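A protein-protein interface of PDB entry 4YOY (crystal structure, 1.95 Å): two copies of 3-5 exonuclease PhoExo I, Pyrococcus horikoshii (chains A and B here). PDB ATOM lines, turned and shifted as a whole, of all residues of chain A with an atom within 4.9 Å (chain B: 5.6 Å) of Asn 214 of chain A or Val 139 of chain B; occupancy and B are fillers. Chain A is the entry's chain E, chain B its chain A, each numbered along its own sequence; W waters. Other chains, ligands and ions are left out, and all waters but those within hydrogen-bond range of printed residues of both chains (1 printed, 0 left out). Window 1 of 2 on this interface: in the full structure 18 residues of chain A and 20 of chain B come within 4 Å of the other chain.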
ATOM      1  N   LEU A  13     -14.787  13.273   3.070  1.00  0.00           N
ATOM      2  CA  LEU A  13     -16.128  13.170   2.505  1.00  0.00           C
ATOM      3  C   LEU A  13     -16.733  11.817   2.846  1.00  0.00           C
ATOM      4  O   LEU A  13     -16.006  10.834   2.943  1.00  0.00           O
ATOM      5  CB  LEU A  13     -16.098  13.359   0.974  1.00  0.00           C
ATOM      6  CG  LEU A  13     -15.368  14.569   0.382  1.00  0.00           C
ATOM      7  CD1 LEU A  13     -15.417  14.514  -1.138  1.00  0.00           C
ATOM      8  CD2 LEU A  13     -15.984  15.861   0.874  1.00  0.00           C
ATOM      9  N   PHE A  17     -20.297  12.014  -1.067  1.00  0.00           N
ATOM     10  CA  PHE A  17     -19.456  13.189  -1.336  1.00  0.00           C
ATOM     11  C   PHE A  17     -19.834  14.376  -0.462  1.00  0.00           C
ATOM     12  O   PHE A  17     -19.538  15.519  -0.793  1.00  0.00           O
ATOM     13  CB  PHE A  17     -19.500  13.593  -2.823  1.00  0.00           C
ATOM     14  CG  PHE A  17     -19.047  12.505  -3.752  1.00  0.00           C
ATOM     15  CD1 PHE A  17     -17.703  12.179  -3.845  1.00  0.00           C
ATOM     16  CD2 PHE A  17     -19.960  11.805  -4.527  1.00  0.00           C
ATOM     17  CE1 PHE A  17     -17.278  11.171  -4.688  1.00  0.00           C
ATOM     18  CE2 PHE A  17     -19.541  10.789  -5.369  1.00  0.00           C
ATOM     19  CZ  PHE A  17     -18.197  10.474  -5.449  1.00  0.00           C
ATOM     20  N   TYR A 212     -10.302  12.168  -9.168  1.00  0.00           N
ATOM     21  CA  TYR A 212     -11.361  12.411 -10.149  1.00  0.00           C
ATOM     22  C   TYR A 212     -12.267  13.559  -9.705  1.00  0.00           C
ATOM     23  O   TYR A 212     -12.233  13.964  -8.543  1.00  0.00           O
ATOM     24  CB  TYR A 212     -12.160  11.125 -10.392  1.00  0.00           C
ATOM     25  CG  TYR A 212     -12.726  10.500  -9.128  1.00  0.00           C
ATOM     26  CD1 TYR A 212     -13.915  10.957  -8.585  1.00  0.00           C
ATOM     27  CD2 TYR A 212     -12.067   9.460  -8.485  1.00  0.00           C
ATOM     28  CE1 TYR A 212     -14.436  10.407  -7.434  1.00  0.00           C
ATOM     29  CE2 TYR A 212     -12.589   8.891  -7.310  1.00  0.00           C
ATOM     30  CZ  TYR A 212     -13.776   9.376  -6.799  1.00  0.00           C
ATOM     31  OH  TYR A 212     -14.329   8.839  -5.660  1.00  0.00           O
ATOM     32  N   PRO A 213     -13.069  14.103 -10.637  1.00  0.00           N
ATOM     33  CA  PRO A 213     -13.973  15.203 -10.275  1.00  0.00           C
ATOM     34  C   PRO A 213     -15.021  14.823  -9.233  1.00  0.00           C
ATOM     35  O   PRO A 213     -15.639  13.776  -9.347  1.00  0.00           O
ATOM     36  CB  PRO A 213     -14.660  15.548 -11.610  1.00  0.00           C
ATOM     37  CG  PRO A 213     -13.664  15.104 -12.674  1.00  0.00           C
ATOM     38  CD  PRO A 213     -13.076  13.831 -12.088  1.00  0.00           C
ATOM     39  N   ASN A 214     -15.196  15.667  -8.226  1.00  0.00           N
ATOM     40  CA  ASN A 214     -16.362  15.596  -7.352  1.00  0.00           C
ATOM     41  C   ASN A 214     -17.611  15.845  -8.189  1.00  0.00           C
ATOM     42  O   ASN A 214     -17.772  16.931  -8.725  1.00  0.00           O
ATOM     43  CB  ASN A 214     -16.246  16.634  -6.235  1.00  0.00           C
ATOM     44  CG  ASN A 214     -17.347  16.507  -5.191  1.00  0.00           C
ATOM     45  OD1 ASN A 214     -18.477  16.121  -5.494  1.00  0.00           O
ATOM     46  ND2 ASN A 214     -17.009  16.828  -3.945  1.00  0.00           N
ATOM     47  N   PRO A 215     -18.500  14.844  -8.312  1.00  0.00           N
ATOM     48  CA  PRO A 215     -19.610  15.043  -9.252  1.00  0.00           C
ATOM     49  C   PRO A 215     -20.602  16.099  -8.769  1.00  0.00           C
ATOM     50  O   PRO A 215     -21.405  16.587  -9.570  1.00  0.00           O
ATOM     51  CB  PRO A 215     -20.260  13.660  -9.324  1.00  0.00           C
ATOM     52  CG  PRO A 215     -19.917  13.015  -8.010  1.00  0.00           C
ATOM     53  CD  PRO A 215     -18.548  13.522  -7.659  1.00  0.00           C
ATOM     54  N   LEU A 216     -20.557  16.441  -7.477  1.00  0.00           N
ATOM     55  CA  LEU A 216     -21.556  17.347  -6.897  1.00  0.00           C
ATOM     56  C   LEU A 216     -21.024  18.770  -6.783  1.00  0.00           C
ATOM     57  O   LEU A 216     -21.782  19.700  -6.508  1.00  0.00           O
ATOM     58  CB  LEU A 216     -22.025  16.833  -5.503  1.00  0.00           C
ATOM     59  CG  LEU A 216     -22.547  15.397  -5.479  1.00  0.00           C
ATOM     60  CD1 LEU A 216     -23.198  15.023  -4.119  1.00  0.00           C
ATOM     61  CD2 LEU A 216     -23.536  15.157  -6.609  1.00  0.00           C
ATOM     62  N   VAL A 217     -19.719  18.935  -6.992  1.00  0.00           N
ATOM     63  CA  VAL A 217     -19.056  20.219  -6.797  1.00  0.00           C
ATOM     64  C   VAL A 217     -18.056  20.472  -7.931  1.00  0.00           C
ATOM     65  O   VAL A 217     -16.866  20.153  -7.824  1.00  0.00           O
ATOM     66  CB  VAL A 217     -18.306  20.301  -5.441  1.00  0.00           C
ATOM     67  CG1 VAL A 217     -17.970  21.746  -5.137  1.00  0.00           C
ATOM     68  CG2 VAL A 217     -19.133  19.677  -4.274  1.00  0.00           C
ATOM     69  N   ARG A 218     -18.558  21.048  -9.015  1.00  0.00           N
ATOM     70  CA  ARG A 218     -17.769  21.268 -10.216  1.00  0.00           C
ATOM     71  C   ARG A 218     -16.491  22.069  -9.907  1.00  0.00           C
ATOM     72  O   ARG A 218     -16.521  22.999  -9.097  1.00  0.00           O
ATOM     73  CB  ARG A 218     -18.637  21.983 -11.262  1.00  0.00           C
ATOM     74  CG  ARG A 218     -18.021  22.048 -12.629  1.00  0.00           C
ATOM     75  CD  ARG A 218     -19.121  22.044 -13.704  1.00  0.00           C
ATOM     76  NE  ARG A 218     -19.592  23.353 -14.129  1.00  0.00           N
ATOM     77  CZ  ARG A 218     -20.851  23.635 -14.471  1.00  0.00           C
ATOM     78  NH1 ARG A 218     -21.152  24.860 -14.883  1.00  0.00           N
ATOM     79  NH2 ARG A 218     -21.819  22.715 -14.374  1.00  0.00           N
ATOM     80  N   PHE A 220     -13.925  20.958  -8.289  1.00  0.00           N
ATOM     81  CA  PHE A 220     -13.225  20.361  -7.136  1.00  0.00           C
ATOM     82  C   PHE A 220     -12.935  18.881  -7.393  1.00  0.00           C
ATOM     83  O   PHE A 220     -13.811  18.152  -7.859  1.00  0.00           O
ATOM     84  CB  PHE A 220     -14.051  20.495  -5.854  1.00  0.00           C
ATOM     85  CG  PHE A 220     -14.157  21.903  -5.329  1.00  0.00           C
ATOM     86  CD1 PHE A 220     -14.905  22.862  -6.008  1.00  0.00           C
ATOM     87  CD2 PHE A 220     -13.555  22.252  -4.134  1.00  0.00           C
ATOM     88  CE1 PHE A 220     -15.023  24.143  -5.520  1.00  0.00           C
ATOM     89  CE2 PHE A 220     -13.676  23.534  -3.631  1.00  0.00           C
ATOM     90  CZ  PHE A 220     -14.420  24.482  -4.322  1.00  0.00           C
ATOM     91  N   MET A 221     -11.723  18.429  -7.066  1.00  0.00           N
ATOM     92  CA  MET A 221     -11.349  17.032  -7.288  1.00  0.00           C
ATOM     93  C   MET A 221     -11.468  16.226  -5.987  1.00  0.00           C
ATOM     94  O   MET A 221     -11.393  16.782  -4.888  1.00  0.00           O
ATOM     95  CB  MET A 221      -9.916  16.917  -7.837  1.00  0.00           C
ATOM     96  CG  MET A 221      -9.666  17.726  -9.130  1.00  0.00           C
ATOM     97  SD  MET A 221     -10.746  17.208 -10.494  1.00  0.00           S
ATOM     98  CE  MET A 221     -11.621  18.732 -10.886  1.00  0.00           C
ATOM     99  N   VAL A 222     -11.624  14.914  -6.133  1.00  0.00           N
ATOM    100  CA  VAL A 222     -11.642  13.988  -5.005  1.00  0.00           C
ATOM    101  C   VAL A 222     -10.407  13.096  -5.064  1.00  0.00           C
ATOM    102  O   VAL A 222     -10.051  12.570  -6.120  1.00  0.00           O
ATOM    103  CB  VAL A 222     -12.894  13.098  -5.009  1.00  0.00           C
ATOM    104  CG1 VAL A 222     -12.865  12.104  -3.831  1.00  0.00           C
ATOM    105  CG2 VAL A 222     -14.156  13.942  -4.970  1.00  0.00           C
ATOM    106  N   TYR B  34     -16.610  10.074 -13.410  1.00  0.00           N
ATOM    107  CA  TYR B  34     -17.355  11.322 -13.605  1.00  0.00           C
ATOM    108  C   TYR B  34     -16.683  12.283 -14.567  1.00  0.00           C
ATOM    109  O   TYR B  34     -16.668  13.493 -14.326  1.00  0.00           O
ATOM    110  CB  TYR B  34     -17.576  12.026 -12.253  1.00  0.00           C
ATOM    111  CG  TYR B  34     -18.108  11.084 -11.177  1.00  0.00           C
ATOM    112  CD1 TYR B  34     -19.422  10.639 -11.194  1.00  0.00           C
ATOM    113  CD2 TYR B  34     -17.271  10.617 -10.168  1.00  0.00           C
ATOM    114  CE1 TYR B  34     -19.899   9.757 -10.214  1.00  0.00           C
ATOM    115  CE2 TYR B  34     -17.732   9.745  -9.190  1.00  0.00           C
ATOM    116  CZ  TYR B  34     -19.044   9.321  -9.215  1.00  0.00           C
ATOM    117  OH  TYR B  34     -19.474   8.453  -8.233  1.00  0.00           O
ATOM    118  N   LYS B  35     -16.113  11.746 -15.645  1.00  0.00           N
ATOM    119  CA  LYS B  35     -15.462  12.585 -16.654  1.00  0.00           C
ATOM    120  C   LYS B  35     -16.189  12.536 -17.992  1.00  0.00           C
ATOM    121  O   LYS B  35     -16.078  13.466 -18.771  1.00  0.00           O
ATOM    122  CB  LYS B  35     -13.991  12.180 -16.858  1.00  0.00           C
ATOM    123  CG  LYS B  35     -13.082  12.473 -15.671  1.00  0.00           C
ATOM    124  CD  LYS B  35     -11.682  11.851 -15.880  1.00  0.00           C
ATOM    125  CE  LYS B  35     -10.735  12.216 -14.746  1.00  0.00           C
ATOM    126  NZ  LYS B  35      -9.354  11.698 -14.948  1.00  0.00           N
ATOM    127  N   HIS B  78     -29.951  14.945 -11.981  1.00  0.00           N
ATOM    128  CA  HIS B  78     -29.524  16.337 -11.901  1.00  0.00           C
ATOM    129  C   HIS B  78     -30.172  17.128 -13.021  1.00  0.00           C
ATOM    130  O   HIS B  78     -30.034  16.780 -14.193  1.00  0.00           O
ATOM    131  CB  HIS B  78     -27.989  16.471 -11.985  1.00  0.00           C
ATOM    132  CG  HIS B  78     -27.277  16.073 -10.736  1.00  0.00           C
ATOM    133  ND1 HIS B  78     -25.901  16.168 -10.600  1.00  0.00           N
ATOM    134  CD2 HIS B  78     -27.734  15.585  -9.547  1.00  0.00           C
ATOM    135  CE1 HIS B  78     -25.550  15.761  -9.389  1.00  0.00           C
ATOM    136  NE2 HIS B  78     -26.647  15.393  -8.735  1.00  0.00           N
ATOM    137  N   SER B 137     -23.443  23.584 -10.309  1.00  0.00           N
ATOM    138  CA  SER B 137     -22.601  22.883  -9.360  1.00  0.00           C
ATOM    139  C   SER B 137     -22.312  21.461  -9.838  1.00  0.00           C
ATOM    140  O   SER B 137     -21.367  20.825  -9.372  1.00  0.00           O
ATOM    141  CB  SER B 137     -23.290  22.860  -7.982  1.00  0.00           C
ATOM    142  OG  SER B 137     -22.413  22.424  -6.972  1.00  0.00           O
ATOM    143  N   SER B 138     -23.126  20.967 -10.769  1.00  0.00           N
ATOM    144  CA  SER B 138     -23.106  19.547 -11.147  1.00  0.00           C
ATOM    145  C   SER B 138     -22.126  19.221 -12.270  1.00  0.00           C
ATOM    146  O   SER B 138     -22.166  19.849 -13.311  1.00  0.00           O
ATOM    147  CB  SER B 138     -24.514  19.098 -11.560  1.00  0.00           C
ATOM    148  OG  SER B 138     -24.519  17.802 -12.148  1.00  0.00           O
ATOM    149  N   VAL B 139     -21.267  18.221 -12.070  1.00  0.00           N
ATOM    150  CA  VAL B 139     -20.434  17.747 -13.166  1.00  0.00           C
ATOM    151  C   VAL B 139     -21.261  16.934 -14.192  1.00  0.00           C
ATOM    152  O   VAL B 139     -21.080  17.119 -15.390  1.00  0.00           O
ATOM    153  CB  VAL B 139     -19.222  16.925 -12.648  1.00  0.00           C
ATOM    154  CG1 VAL B 139     -18.481  16.279 -13.815  1.00  0.00           C
ATOM    155  CG2 VAL B 139     -18.281  17.833 -11.882  1.00  0.00           C
ATOM    156  N   PRO B 140     -22.170  16.039 -13.742  1.00  0.00           N
ATOM    157  CA  PRO B 140     -23.012  15.406 -14.774  1.00  0.00           C
ATOM    158  C   PRO B 140     -23.771  16.405 -15.689  1.00  0.00           C
ATOM    159  O   PRO B 140     -23.935  16.149 -16.884  1.00  0.00           O
ATOM    160  CB  PRO B 140     -23.990  14.562 -13.943  1.00  0.00           C
ATOM    161  CG  PRO B 140     -23.112  14.119 -12.759  1.00  0.00           C
ATOM    162  CD  PRO B 140     -22.309  15.352 -12.432  1.00  0.00           C
ATOM    163  N   VAL B 141     -24.216  17.528 -15.144  1.00  0.00           N
ATOM    164  CA  VAL B 141     -24.878  18.534 -15.975  1.00  0.00           C
ATOM    165  C   VAL B 141     -23.908  19.115 -17.017  1.00  0.00           C
ATOM    166  O   VAL B 141     -24.262  19.269 -18.187  1.00  0.00           O
ATOM    167  CB  VAL B 141     -25.473  19.670 -15.124  1.00  0.00           C
ATOM    168  CG1 VAL B 141     -25.812  20.866 -16.021  1.00  0.00           C
ATOM    169  CG2 VAL B 141     -26.773  19.147 -14.364  1.00  0.00           C
ATOM    170  N   ARG B 142     -22.677  19.386 -16.597  1.00  0.00           N
ATOM    171  CA  ARG B 142     -21.653  19.907 -17.522  1.00  0.00           C
ATOM    172  C   ARG B 142     -21.314  18.871 -18.613  1.00  0.00           C
ATOM    173  O   ARG B 142     -21.102  19.229 -19.778  1.00  0.00           O
ATOM    174  CB  ARG B 142     -20.392  20.304 -16.753  1.00  0.00           C
ATOM    175  CG  ARG B 142     -19.200  20.725 -17.658  1.00  0.00           C
ATOM    176  CD  ARG B 142     -19.528  21.910 -18.545  1.00  0.00           C
ATOM    177  NE  ARG B 142     -18.294  22.384 -19.213  1.00  0.00           N
ATOM    178  CZ  ARG B 142     -18.242  23.221 -20.254  1.00  0.00           C
ATOM    179  NH1 ARG B 142     -19.353  23.711 -20.829  1.00  0.00           N
ATOM    180  NH2 ARG B 142     -17.051  23.550 -20.752  1.00  0.00           N
ATOM    181  N   ILE B 143     -21.306  17.589 -18.252  1.00  0.00           N
ATOM    182  CA  ILE B 143     -21.099  16.521 -19.239  1.00  0.00           C
ATOM    183  C   ILE B 143     -22.270  16.426 -20.230  1.00  0.00           C
ATOM    184  O   ILE B 143     -22.046  16.279 -21.441  1.00  0.00           O
ATOM    185  CB  ILE B 143     -20.858  15.181 -18.554  1.00  0.00           C
ATOM    186  CG1 ILE B 143     -19.492  15.204 -17.856  1.00  0.00           C
ATOM    187  CG2 ILE B 143     -20.929  14.016 -19.550  1.00  0.00           C
ATOM    188  CD1 ILE B 143     -19.294  14.055 -16.855  1.00  0.00           C
ATOM    189  N   ALA B 144     -23.513  16.559 -19.752  1.00  0.00           N
ATOM    190  CA  ALA B 144     -24.652  16.662 -20.662  1.00  0.00           C
ATOM    191  C   ALA B 144     -24.503  17.864 -21.615  1.00  0.00           C
ATOM    192  O   ALA B 144     -24.850  17.782 -22.783  1.00  0.00           O
ATOM    193  CB  ALA B 144     -25.992  16.777 -19.858  1.00  0.00           C
ATOM    194  N   GLU B 192     -11.956  21.862 -14.618  1.00  0.00           N
ATOM    195  CA  GLU B 192     -13.055  20.898 -14.488  1.00  0.00           C
ATOM    196  C   GLU B 192     -12.554  19.448 -14.435  1.00  0.00           C
ATOM    197  O   GLU B 192     -13.338  18.522 -14.224  1.00  0.00           O
ATOM    198  CB  GLU B 192     -14.066  21.076 -15.630  1.00  0.00           C
ATOM    199  CG  GLU B 192     -14.760  22.440 -15.584  1.00  0.00           C
ATOM    200  CD  GLU B 192     -15.877  22.625 -16.625  1.00  0.00           C
ATOM    201  OE1 GLU B 192     -16.780  23.454 -16.339  1.00  0.00           O
ATOM    202  OE2 GLU B 192     -15.850  21.975 -17.712  1.00  0.00           O
ATOM    203  N   LEU B 195     -13.206  16.927 -18.551  1.00  0.00           N
ATOM    204  CA  LEU B 195     -14.509  16.450 -18.976  1.00  0.00           C
ATOM    205  C   LEU B 195     -14.582  16.358 -20.498  1.00  0.00           C
ATOM    206  O   LEU B 195     -14.088  17.246 -21.210  1.00  0.00           O
ATOM    207  CB  LEU B 195     -15.603  17.377 -18.440  1.00  0.00           C
ATOM    208  CG  LEU B 195     -15.534  17.641 -16.929  1.00  0.00           C
ATOM    209  CD1 LEU B 195     -16.677  18.557 -16.488  1.00  0.00           C
ATOM    210  CD2 LEU B 195     -15.554  16.332 -16.113  1.00  0.00           C
HETATM  211  O   HOH W   1     -18.971  24.954 -16.581  1.00  0.00           O
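The side-chain hydroxyl of Ser 137 of chain B lies within hydrogen-bond range of the backbone carbonyl oxygen of Leu 216 of chain A, 2.8 Å away.
The backbone NH (N) of Val 217 of chain A is in hydrogen-bond range of the backbone carbonyl oxygen (O) of Ser 137 of chain B.
The backbone carbonyl oxygen of Ser 137 of chain B sits at hydrogen-bond distance from the backbone NH of Arg 218 of chain A (2.8 Å).
NH2 of Arg 218 of chain A sits at hydrogen-bond distance from O of Ser 138 of chain B (3.1 Å).
The backbone carbonyl oxygen of Pro 215 of chain A sits at hydrogen-bond distance from the backbone NH of Val 139 of chain B.
NE of Arg 218 of chain A lies within salt-bridge range of OE1 of Glu 192 of chain B (3.6 Å).
A ring nitrogen (ND1) of His 78 of chain B is in hydrogen-bond range of the side-chain hydroxyl (OG) of Ser 138 of chain B, at 2.6 Å.
OG of Ser 138 of chain B lies within hydrogen-bond range of N of Val 141 of chain B, 3.0 Å away.
The side-chain carboxylate (OE2) of Glu 192 of chain B lies within salt-bridge range of the guanidinium group (NE) of Arg 142 of chain B (2.9 Å).
The backbone carbonyl oxygen (O) of Tyr 212 of chain A sits at hydrogen-bond distance from the backbone NH (N) of Val 222 of chain A (2.7 Å).
The side-chain amide oxygen (OD1) of Asn 214 of chain A lies within hydrogen-bond range of the backbone NH (N) of Val 217 of chain A.
N of Asn 214 of chain A lies within hydrogen-bond range of O of Phe 220 of chain A.
Tyr 34 of chain B touches Tyr 212 of chain A (CD2 to CD1, 3.7 Å).
Pro 213 of chain A touches Tyr 34 of chain B (O to CD2, 3.6 Å).
O of Glu 192 of chain B touches CG of Pro 213 of chain A (3.8 Å).
O of Asn 214 of chain A touches CG2 of Val 139 of chain B, at 3.3 Å.
Pro 215 of chain A touches Tyr 34 of chain B (CB to CD1, 3.7 Å).
Ser 138 of chain B touches Pro 215 of chain A.
O of Pro 215 of chain A touches CD of Pro 140 of chain B, 3.2 Å away.
CE1 of His 78 of chain B touches CD2 of Leu 216 of chain A (3.5 Å).
Arg 218 of chain A touches Val 139 of chain B (CA to CG2, 3.9 Å).
Met 221 of chain A touches Glu 192 of chain B.
Asn 214 of chain A touches one residue of chain B.
Of the printed residues of chain B, Arg 218 of chain A touches Ser 137, Ser 138, Val 139, Arg 142 and Glu 192.
Phe 220 of chain A touches none of the printed residues of chain B.
Of the printed residues of chain A, Lys 35 of chain B touches Pro 213.
Of the printed residues of chain A, His 78 of chain B touches Leu 216.
Of the printed residues of chain A, Ser 138 of chain B touches Pro 215 (3.8 Å) and Arg 218 (3.1 Å).
Of chain A, only Asn 214 (3.3 Å), Pro 215 (3.0 Å) and Arg 218 (3.9 Å) come within 4 Å of Val 139 of chain B.
Leu 195 of chain B touches none of the printed residues of chain A.
The nearest residue of chain B that does not touch Asn 214 of chain A is Ser 137 of chain B (5.3 Å).
The nearest printed residue of chain B that does not touch Val 217 of chain A is Val 139 of chain B (4.8 Å).
Of the 12 printed residues of chain A, 9 touch a printed residue of chain B.
Printed residues of chain A that touch a printed residue of chain B: Phe 17, Tyr 212, Pro 213, Asn 214, Pro 215, Leu 216, Val 217, Arg 218 and Met 221.
Hydrophobic or aromatic side chains of chain A that line the printed part of chain B: Phe 17, Tyr 212, Pro 213, Pro 215, Leu 216 and Met 221.
Printed residues of chain B that touch a printed residue of chain A: Tyr 34, Lys 35, His 78, Ser 137, Ser 138, Val 139, Pro 140, Arg 142 and Glu 192.
Hydrophobic or aromatic side chains of chain B that line the printed part of chain A: Tyr 34, His 78, Val 139 and Pro 140.
No position is printed for both chains.
Water W1 bridges the side-chain carboxylate (OE1) of Glu 192 of chain B (2.7 Å) and the guanidinium group (NH1) of Arg 218 of chain A (2.8 Å).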
